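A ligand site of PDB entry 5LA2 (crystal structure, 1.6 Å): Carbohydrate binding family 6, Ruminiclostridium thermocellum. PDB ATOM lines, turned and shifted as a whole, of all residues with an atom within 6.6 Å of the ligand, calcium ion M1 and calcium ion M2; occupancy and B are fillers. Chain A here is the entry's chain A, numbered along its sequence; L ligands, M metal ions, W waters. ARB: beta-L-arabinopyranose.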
ATOM      1  N   TYR A 358      -9.647 -31.860  -9.122  1.00  0.00           N
ATOM      2  CA  TYR A 358      -8.385 -32.045  -9.788  1.00  0.00           C
ATOM      3  C   TYR A 358      -7.411 -31.036  -9.187  1.00  0.00           C
ATOM      4  O   TYR A 358      -7.662 -29.808  -9.219  1.00  0.00           O
ATOM      5  CB  TYR A 358      -8.506 -31.849 -11.297  1.00  0.00           C
ATOM      6  CG  TYR A 358      -7.168 -31.668 -12.003  1.00  0.00           C
ATOM      7  CD1 TYR A 358      -6.084 -32.522 -11.748  1.00  0.00           C
ATOM      8  CD2 TYR A 358      -6.994 -30.640 -12.906  1.00  0.00           C
ATOM      9  CE1 TYR A 358      -4.863 -32.348 -12.387  1.00  0.00           C
ATOM     10  CE2 TYR A 358      -5.788 -30.467 -13.558  1.00  0.00           C
ATOM     11  CZ  TYR A 358      -4.722 -31.301 -13.286  1.00  0.00           C
ATOM     12  OH  TYR A 358      -3.535 -31.117 -13.948  1.00  0.00           O
ATOM     13  N   ASP A 359      -6.345 -31.571  -8.605  1.00  0.00           N
ATOM     14  CA  ASP A 359      -5.228 -30.756  -8.183  1.00  0.00           C
ATOM     15  C   ASP A 359      -3.956 -31.144  -8.913  1.00  0.00           C
ATOM     16  O   ASP A 359      -3.731 -32.339  -9.163  1.00  0.00           O
ATOM     17  CB  ASP A 359      -5.023 -30.860  -6.668  1.00  0.00           C
ATOM     18  CG  ASP A 359      -4.396 -29.616  -6.128  1.00  0.00           C
ATOM     19  OD1 ASP A 359      -5.167 -28.679  -5.803  1.00  0.00           O
ATOM     20  OD2 ASP A 359      -3.135 -29.551  -6.026  1.00  0.00           O
ATOM     21  N   THR A 360      -3.141 -30.156  -9.237  1.00  0.00           N
ATOM     22  CA  THR A 360      -1.938 -30.392 -10.069  1.00  0.00           C
ATOM     23  C   THR A 360      -0.817 -31.146  -9.366  1.00  0.00           C
ATOM     24  O   THR A 360       0.041 -31.717 -10.035  1.00  0.00           O
ATOM     25  CB  THR A 360      -1.335 -29.083 -10.605  1.00  0.00           C
ATOM     26  OG1 THR A 360      -0.958 -28.241  -9.502  1.00  0.00           O
ATOM     27  CG2 THR A 360      -2.327 -28.382 -11.528  1.00  0.00           C
ATOM     28  N   ASP A 361      -0.822 -31.160  -8.045  1.00  0.00           N
ATOM     29  CA  ASP A 361       0.109 -31.989  -7.265  1.00  0.00           C
ATOM     30  C   ASP A 361      -0.647 -32.719  -6.179  1.00  0.00           C
ATOM     31  O   ASP A 361      -1.564 -32.157  -5.578  1.00  0.00           O
ATOM     32  CB  ASP A 361       1.352 -31.221  -6.738  1.00  0.00           C
ATOM     33  CG  ASP A 361       1.036 -29.852  -6.129  1.00  0.00           C
ATOM     34  OD1 ASP A 361       0.009 -29.680  -5.449  1.00  0.00           O
ATOM     35  OD2 ASP A 361       1.865 -28.927  -6.302  1.00  0.00           O
ATOM     36  N   SER A 362      -0.282 -33.979  -5.928  1.00  0.00           N
ATOM     37  CA  SER A 362      -1.046 -34.785  -4.988  1.00  0.00           C
ATOM     38  C   SER A 362      -0.742 -34.416  -3.532  1.00  0.00           C
ATOM     39  O   SER A 362      -1.529 -34.714  -2.656  1.00  0.00           O
ATOM     40  CB  SER A 362      -0.798 -36.257  -5.222  1.00  0.00           C
ATOM     41  OG  SER A 362       0.556 -36.511  -5.088  1.00  0.00           O
ATOM     42  N   VAL A 363       0.383 -33.779  -3.263  1.00  0.00           N
ATOM     43  CA  VAL A 363       0.597 -33.222  -1.919  1.00  0.00           C
ATOM     44  C   VAL A 363      -0.433 -32.112  -1.625  1.00  0.00           C
ATOM     45  O   VAL A 363      -0.843 -31.388  -2.526  1.00  0.00           O
ATOM     46  CB  VAL A 363       2.049 -32.690  -1.767  1.00  0.00           C
ATOM     47  CG1 VAL A 363       2.286 -31.454  -2.611  1.00  0.00           C
ATOM     48  CG2 VAL A 363       2.392 -32.443  -0.299  1.00  0.00           C
ATOM     49  N   ASN A 364      -0.885 -32.024  -0.380  1.00  0.00           N
ATOM     50  CA  ASN A 364      -1.603 -30.856   0.103  1.00  0.00           C
ATOM     51  C   ASN A 364      -0.542 -29.885   0.644  1.00  0.00           C
ATOM     52  O   ASN A 364      -0.066 -30.029   1.773  1.00  0.00           O
ATOM     53  CB  ASN A 364      -2.588 -31.298   1.173  1.00  0.00           C
ATOM     54  CG  ASN A 364      -3.266 -30.134   1.876  1.00  0.00           C
ATOM     55  OD1 ASN A 364      -2.879 -28.969   1.727  1.00  0.00           O
ATOM     56  ND2 ASN A 364      -4.253 -30.457   2.674  1.00  0.00           N
ATOM     57  N   VAL A 365      -0.180 -28.880  -0.136  1.00  0.00           N
ATOM     58  CA  VAL A 365       1.024 -28.064   0.209  1.00  0.00           C
ATOM     59  C   VAL A 365       0.834 -27.266   1.508  1.00  0.00           C
ATOM     60  O   VAL A 365       1.760 -27.109   2.294  1.00  0.00           O
ATOM     61  CB  VAL A 365       1.484 -27.132  -0.946  1.00  0.00           C
ATOM     62  CG1 VAL A 365       1.693 -27.874  -2.256  1.00  0.00           C
ATOM     63  CG2 VAL A 365       0.496 -26.060  -1.190  1.00  0.00           C
ATOM     64  N   GLU A 373      -5.564 -35.717   0.924  1.00  0.00           N
ATOM     65  CA  GLU A 373      -6.040 -35.408  -0.425  1.00  0.00           C
ATOM     66  C   GLU A 373      -5.213 -34.277  -1.036  1.00  0.00           C
ATOM     67  O   GLU A 373      -4.423 -33.626  -0.370  1.00  0.00           O
ATOM     68  CB  GLU A 373      -7.523 -35.072  -0.385  1.00  0.00           C
ATOM     69  CG  GLU A 373      -8.362 -36.276  -0.017  1.00  0.00           C
ATOM     70  CD  GLU A 373      -9.679 -35.902   0.602  1.00  0.00           C
ATOM     71  OE1 GLU A 373      -9.711 -35.569   1.819  1.00  0.00           O
ATOM     72  OE2 GLU A 373     -10.683 -35.949  -0.125  1.00  0.00           O
ATOM     73  N   GLY A 374      -5.372 -34.071  -2.333  1.00  0.00           N
ATOM     74  CA  GLY A 374      -4.472 -33.223  -3.084  1.00  0.00           C
ATOM     75  C   GLY A 374      -4.765 -31.744  -3.094  1.00  0.00           C
ATOM     76  O   GLY A 374      -3.927 -30.961  -3.513  1.00  0.00           O
ATOM     77  N   VAL A 375      -5.962 -31.357  -2.663  1.00  0.00           N
ATOM     78  CA  VAL A 375      -6.319 -29.944  -2.657  1.00  0.00           C
ATOM     79  C   VAL A 375      -5.420 -29.236  -1.629  1.00  0.00           C
ATOM     80  O   VAL A 375      -5.138 -29.765  -0.567  1.00  0.00           O
ATOM     81  CB  VAL A 375      -7.801 -29.758  -2.343  1.00  0.00           C
ATOM     82  CG1 VAL A 375      -8.175 -28.278  -2.268  1.00  0.00           C
ATOM     83  CG2 VAL A 375      -8.631 -30.517  -3.382  1.00  0.00           C
ATOM     84  N   ASP A 376      -4.946 -28.044  -1.975  1.00  0.00           N
ATOM     85  CA  ASP A 376      -4.021 -27.327  -1.107  1.00  0.00           C
ATOM     86  C   ASP A 376      -4.798 -26.422  -0.172  1.00  0.00           C
ATOM     87  O   ASP A 376      -5.502 -25.524  -0.645  1.00  0.00           O
ATOM     88  CB  ASP A 376      -3.006 -26.556  -1.959  1.00  0.00           C
ATOM     89  CG  ASP A 376      -2.325 -27.479  -2.950  1.00  0.00           C
ATOM     90  OD1 ASP A 376      -1.817 -28.553  -2.489  1.00  0.00           O
ATOM     91  OD2 ASP A 376      -2.396 -27.229  -4.183  1.00  0.00           O
ATOM     92  N   GLU A 378      -4.910 -24.322   3.673  1.00  0.00           N
ATOM     93  CA  GLU A 378      -4.232 -23.565   4.742  1.00  0.00           C
ATOM     94  C   GLU A 378      -5.263 -22.940   5.707  1.00  0.00           C
ATOM     95  O   GLU A 378      -6.449 -22.725   5.354  1.00  0.00           O
ATOM     96  CB  GLU A 378      -3.352 -22.455   4.134  1.00  0.00           C
ATOM     97  CG  GLU A 378      -4.121 -21.441   3.268  1.00  0.00           C
ATOM     98  CD  GLU A 378      -3.223 -20.421   2.590  1.00  0.00           C
ATOM     99  OE1 GLU A 378      -2.093 -20.236   3.054  1.00  0.00           O
ATOM    100  OE2 GLU A 378      -3.659 -19.796   1.595  1.00  0.00           O
ATOM    101  N   ASN A 388      -8.836 -21.951   4.035  1.00  0.00           N
ATOM    102  CA  ASN A 388      -9.102 -21.610   2.651  1.00  0.00           C
ATOM    103  C   ASN A 388      -8.307 -22.568   1.762  1.00  0.00           C
ATOM    104  O   ASN A 388      -7.295 -23.131   2.184  1.00  0.00           O
ATOM    105  CB  ASN A 388      -8.824 -20.144   2.299  1.00  0.00           C
ATOM    106  CG  ASN A 388      -7.343 -19.751   2.402  1.00  0.00           C
ATOM    107  OD1 ASN A 388      -6.883 -19.316   3.453  1.00  0.00           O
ATOM    108  ND2 ASN A 388      -6.592 -19.890   1.297  1.00  0.00           N
ATOM    109  N   VAL A 389      -8.845 -22.795   0.570  1.00  0.00           N
ATOM    110  CA  VAL A 389      -8.117 -23.422  -0.467  1.00  0.00           C
ATOM    111  C   VAL A 389      -7.179 -22.377  -1.074  1.00  0.00           C
ATOM    112  O   VAL A 389      -7.577 -21.247  -1.350  1.00  0.00           O
ATOM    113  CB  VAL A 389      -9.066 -23.990  -1.557  1.00  0.00           C
ATOM    114  CG1 VAL A 389      -8.235 -24.546  -2.710  1.00  0.00           C
ATOM    115  CG2 VAL A 389      -9.974 -25.062  -0.952  1.00  0.00           C
ATOM    116  N   GLY A 390      -5.932 -22.784  -1.264  1.00  0.00           N
ATOM    117  CA  GLY A 390      -4.879 -21.950  -1.783  1.00  0.00           C
ATOM    118  C   GLY A 390      -4.118 -22.698  -2.845  1.00  0.00           C
ATOM    119  O   GLY A 390      -4.452 -23.843  -3.178  1.00  0.00           O
ATOM    120  N   TRP A 391      -3.061 -22.085  -3.350  1.00  0.00           N
ATOM    121  CA  TRP A 391      -2.264 -22.696  -4.462  1.00  0.00           C
ATOM    122  C   TRP A 391      -3.184 -23.265  -5.538  1.00  0.00           C
ATOM    123  O   TRP A 391      -3.103 -24.432  -5.900  1.00  0.00           O
ATOM    124  CB  TRP A 391      -1.330 -23.807  -3.967  1.00  0.00           C
ATOM    125  CG  TRP A 391      -0.384 -23.328  -2.924  1.00  0.00           C
ATOM    126  CD1 TRP A 391       0.885 -22.895  -3.111  1.00  0.00           C
ATOM    127  CD2 TRP A 391      -0.642 -23.236  -1.504  1.00  0.00           C
ATOM    128  NE1 TRP A 391       1.450 -22.571  -1.898  1.00  0.00           N
ATOM    129  CE2 TRP A 391       0.525 -22.759  -0.900  1.00  0.00           C
ATOM    130  CE3 TRP A 391      -1.735 -23.545  -0.698  1.00  0.00           C
ATOM    131  CZ2 TRP A 391       0.616 -22.548   0.488  1.00  0.00           C
ATOM    132  CZ3 TRP A 391      -1.653 -23.348   0.673  1.00  0.00           C
ATOM    133  CH2 TRP A 391      -0.480 -22.847   1.254  1.00  0.00           C
ATOM    134  N   ILE A 392      -4.099 -22.443  -5.985  1.00  0.00           N
ATOM    135  CA  ILE A 392      -5.052 -22.819  -7.014  1.00  0.00           C
ATOM    136  C   ILE A 392      -4.347 -22.488  -8.317  1.00  0.00           C
ATOM    137  O   ILE A 392      -3.989 -21.329  -8.537  1.00  0.00           O
ATOM    138  CB  ILE A 392      -6.360 -22.047  -6.893  1.00  0.00           C
ATOM    139  CG1 ILE A 392      -7.023 -22.307  -5.539  1.00  0.00           C
ATOM    140  CG2 ILE A 392      -7.303 -22.450  -8.033  1.00  0.00           C
ATOM    141  CD1 ILE A 392      -8.397 -21.648  -5.380  1.00  0.00           C
ATOM    142  N   SER A 393      -4.160 -23.517  -9.125  1.00  0.00           N
ATOM    143  CA  SER A 393      -3.478 -23.442 -10.410  1.00  0.00           C
ATOM    144  C   SER A 393      -4.446 -23.581 -11.576  1.00  0.00           C
ATOM    145  O   SER A 393      -5.484 -24.231 -11.484  1.00  0.00           O
ATOM    146  CB  SER A 393      -2.460 -24.562 -10.470  1.00  0.00           C
ATOM    147  OG  SER A 393      -1.570 -24.385  -9.370  1.00  0.00           O
ATOM    148  N   GLU A 396      -7.268 -26.420 -12.479  1.00  0.00           N
ATOM    149  CA  GLU A 396      -7.796 -27.090 -11.319  1.00  0.00           C
ATOM    150  C   GLU A 396      -9.325 -26.933 -11.230  1.00  0.00           C
ATOM    151  O   GLU A 396      -9.936 -26.011 -11.803  1.00  0.00           O
ATOM    152  CB  GLU A 396      -7.089 -26.598 -10.053  1.00  0.00           C
ATOM    153  CG  GLU A 396      -5.678 -27.136  -9.969  1.00  0.00           C
ATOM    154  CD  GLU A 396      -4.988 -26.901  -8.647  1.00  0.00           C
ATOM    155  OE1 GLU A 396      -5.374 -25.999  -7.865  1.00  0.00           O
ATOM    156  OE2 GLU A 396      -4.038 -27.633  -8.363  1.00  0.00           O
ATOM    157  N   PHE A 445      -2.980 -12.341  -0.458  1.00  0.00           N
ATOM    158  CA  PHE A 445      -3.559 -13.670  -0.383  1.00  0.00           C
ATOM    159  C   PHE A 445      -4.437 -13.928   0.833  1.00  0.00           C
ATOM    160  O   PHE A 445      -5.159 -14.940   0.871  1.00  0.00           O
ATOM    161  CB  PHE A 445      -2.485 -14.732  -0.494  1.00  0.00           C
ATOM    162  CG  PHE A 445      -2.041 -14.974  -1.892  1.00  0.00           C
ATOM    163  CD1 PHE A 445      -2.964 -15.376  -2.879  1.00  0.00           C
ATOM    164  CD2 PHE A 445      -0.710 -14.842  -2.250  1.00  0.00           C
ATOM    165  CE1 PHE A 445      -2.557 -15.616  -4.194  1.00  0.00           C
ATOM    166  CE2 PHE A 445      -0.315 -15.070  -3.569  1.00  0.00           C
ATOM    167  CZ  PHE A 445      -1.226 -15.449  -4.541  1.00  0.00           C
ATOM    168  N   GLN A 446      -4.363 -13.061   1.847  1.00  0.00           N
ATOM    169  CA  GLN A 446      -5.356 -13.080   2.930  1.00  0.00           C
ATOM    170  C   GLN A 446      -6.048 -11.743   3.050  1.00  0.00           C
ATOM    171  O   GLN A 446      -6.435 -11.347   4.125  1.00  0.00           O
ATOM    172  CB  GLN A 446      -4.728 -13.528   4.246  1.00  0.00           C
ATOM    173  CG  GLN A 446      -4.150 -14.927   4.196  1.00  0.00           C
ATOM    174  CD  GLN A 446      -5.214 -16.022   4.180  1.00  0.00           C
ATOM    175  OE1 GLN A 446      -6.343 -15.864   4.677  1.00  0.00           O
ATOM    176  NE2 GLN A 446      -4.836 -17.159   3.632  1.00  0.00           N
ATOM    177  N   GLY A 472      -3.941 -18.204  -9.245  1.00  0.00           N
ATOM    178  CA  GLY A 472      -3.589 -16.953  -8.560  1.00  0.00           C
ATOM    179  C   GLY A 472      -4.648 -16.394  -7.619  1.00  0.00           C
ATOM    180  O   GLY A 472      -4.568 -15.250  -7.221  1.00  0.00           O
ATOM    181  N   PHE A 473      -5.666 -17.177  -7.287  1.00  0.00           N
ATOM    182  CA  PHE A 473      -6.636 -16.744  -6.282  1.00  0.00           C
ATOM    183  C   PHE A 473      -6.789 -17.808  -5.207  1.00  0.00           C
ATOM    184  O   PHE A 473      -6.478 -18.970  -5.434  1.00  0.00           O
ATOM    185  CB  PHE A 473      -7.981 -16.375  -6.932  1.00  0.00           C
ATOM    186  CG  PHE A 473      -8.768 -17.557  -7.483  1.00  0.00           C
ATOM    187  CD1 PHE A 473      -8.488 -18.093  -8.740  1.00  0.00           C
ATOM    188  CD2 PHE A 473      -9.825 -18.120  -6.750  1.00  0.00           C
ATOM    189  CE1 PHE A 473      -9.230 -19.163  -9.245  1.00  0.00           C
ATOM    190  CE2 PHE A 473     -10.549 -19.174  -7.261  1.00  0.00           C
ATOM    191  CZ  PHE A 473     -10.248 -19.713  -8.511  1.00  0.00           C
ATOM    192  N   ASN A 474      -7.249 -17.379  -4.041  1.00  0.00           N
ATOM    193  CA  ASN A 474      -7.612 -18.262  -2.936  1.00  0.00           C
ATOM    194  C   ASN A 474      -9.122 -18.225  -2.812  1.00  0.00           C
ATOM    195  O   ASN A 474      -9.782 -17.252  -3.221  1.00  0.00           O
ATOM    196  CB  ASN A 474      -7.014 -17.775  -1.627  1.00  0.00           C
ATOM    197  CG  ASN A 474      -5.526 -17.943  -1.569  1.00  0.00           C
ATOM    198  OD1 ASN A 474      -4.925 -18.713  -2.329  1.00  0.00           O
ATOM    199  ND2 ASN A 474      -4.892 -17.231  -0.640  1.00  0.00           N
HETATM  200  C1  ARB L   1       0.071 -19.272  -2.802  1.00  0.00           C
HETATM  201  C2  ARB L   1      -1.154 -19.415  -1.899  1.00  0.00           C
HETATM  202  C3  ARB L   1      -1.149 -18.383  -0.813  1.00  0.00           C
HETATM  203  C4  ARB L   1       0.140 -18.422   0.000  1.00  0.00           C
HETATM  204  C5  ARB L   1       1.294 -19.031  -0.762  1.00  0.00           C
HETATM  205  O1  ARB L   1      -0.304 -18.569  -3.986  1.00  0.00           O
HETATM  206  O2  ARB L   1      -2.382 -19.389  -2.644  1.00  0.00           O
HETATM  207  O3  ARB L   1      -2.260 -18.463   0.065  1.00  0.00           O
HETATM  208  O4  ARB L   1      -0.046 -19.140   1.238  1.00  0.00           O
HETATM  209  O5  ARB L   1       1.190 -18.605  -2.135  1.00  0.00           O
HETATM  210 CA    CA M   1      -3.651 -26.776  -6.076  1.00  0.00          CA
HETATM  211 CA    CA M   2      -1.839 -30.194  -4.233  1.00  0.00          CA
HETATM  212  O   HOH W   1      -1.525 -26.662  -7.289  1.00  0.00           O
HETATM  213  O   HOH W   2      -3.827 -19.653  -5.250  1.00  0.00           O
HETATM  214  O   HOH W   3      -5.351 -26.135  -4.417  1.00  0.00           O
HETATM  215  O   HOH W   4      -1.967 -16.995   2.706  1.00  0.00           O
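N of Trp 391 lies within hydrogen-bond range of O2 of the ligand, 2.9 Å away.
The side-chain carboxylate (OE2) of Glu 378 sits at hydrogen-bond distance from an oxygen (O3) of the ligand, 2.5 Å away.
An oxygen (O2) of the ligand sits at hydrogen-bond distance from the side-chain amide oxygen (OD1) of Asn 474, 2.7 Å away.
The backbone carbonyl oxygen of Asp 376 sits at hydrogen-bond distance from the backbone NH of Gly 390 (2.8 Å).
OD1 of Asp 376 lies close to N of Val 365 (2.9 Å).
The backbone NH of Asn 388 is in hydrogen-bond range of the backbone carbonyl oxygen of Glu 378 (2.8 Å).
OE1 of Glu 396 lies close to N of Ser 393, at 3.0 Å.
The backbone NH (N) of Thr 360 sits close to the side-chain carboxylate (OE2) of Glu 396, 2.8 Å away.
The side-chain amide nitrogen (ND2) of Asn 474 is in hydrogen-bond range of the backbone carbonyl oxygen (O) of Phe 445.
Gly 390 touches the ligand.
Phe 445 touches the ligand (CZ to O1, 3.3 Å).
Hydrophobic or aromatic side chains within 4 Å of the ligand: Trp 391 and Phe 445.
Of the 25 residues printed, 5 come within 4 Å of the ligand.
Along chain A the residues within 4 Å of the ligand span positions 378 to 474.
Four residues have an atom within 4 Å of calcium ion M1: Asp 359, Asp 376, Trp 391 and Glu 396.
Of the 25 residues printed, 5 come within 4 Å of calcium ion M2.
Calcium ion M1 is bound by OD2 of Asp 376 (2.3 Å).
O of Trp 391 binds calcium ion M1, 2.4 Å away.
Calcium ion M1 is bound by OD1 of Asp 359 (2.4 Å).
Water W1 is bound to calcium ion M1 (2.5 Å).
Calcium ion M1 is bound by water W3, 2.5 Å away.
OE2 of Glu 396 is bound to calcium ion M1, 2.5 Å away.
Calcium ion M1 is bound by OE1 of Glu 396, 2.6 Å away.
OD2 of Asp 359 binds calcium ion M1 (2.8 Å).
Calcium ion M2 is bound by the side-chain carboxylate (OD1) of Asp 361 (2.3 Å), the side-chain carboxylate (OD2) of Asp 359 (2.3 Å), the backbone carbonyl oxygen (O) of Val 363 (2.3 Å), the backbone carbonyl oxygen (O) of Gly 374 (2.3 Å), the backbone carbonyl oxygen (O) of Asp 361 (2.4 Å) and the side-chain carboxylate (OD1) of Asp 376 (2.4 Å).
Calcium ion M2 has six donor atoms within binding distance.
Slightly farther from calcium ion M2 lies OD2 of Asp 376 (3.0 Å).
Water W3 lies within hydrogen-bond range of O of Gly 390 and N of Asp 376.
Water W1 bridges OG1 of Thr 360 and OG of Ser 393.
Water W2 lies within hydrogen-bond range of the backbone carbonyl oxygen (O) of Phe 473 (2.7 Å), the backbone NH (N) of Ile 392 (2.9 Å), an oxygen (O2) of the ligand (3.0 Å), the backbone NH (N) of Trp 391 (3.2 Å) and the side-chain amide oxygen (OD1) of Asn 474 (3.3 Å).
Water W4 lies within hydrogen-bond range of NE2 of Gln 446 (3.0 Å), O3 of the ligand (3.0 Å) and OE1 of Glu 378 (3.3 Å).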
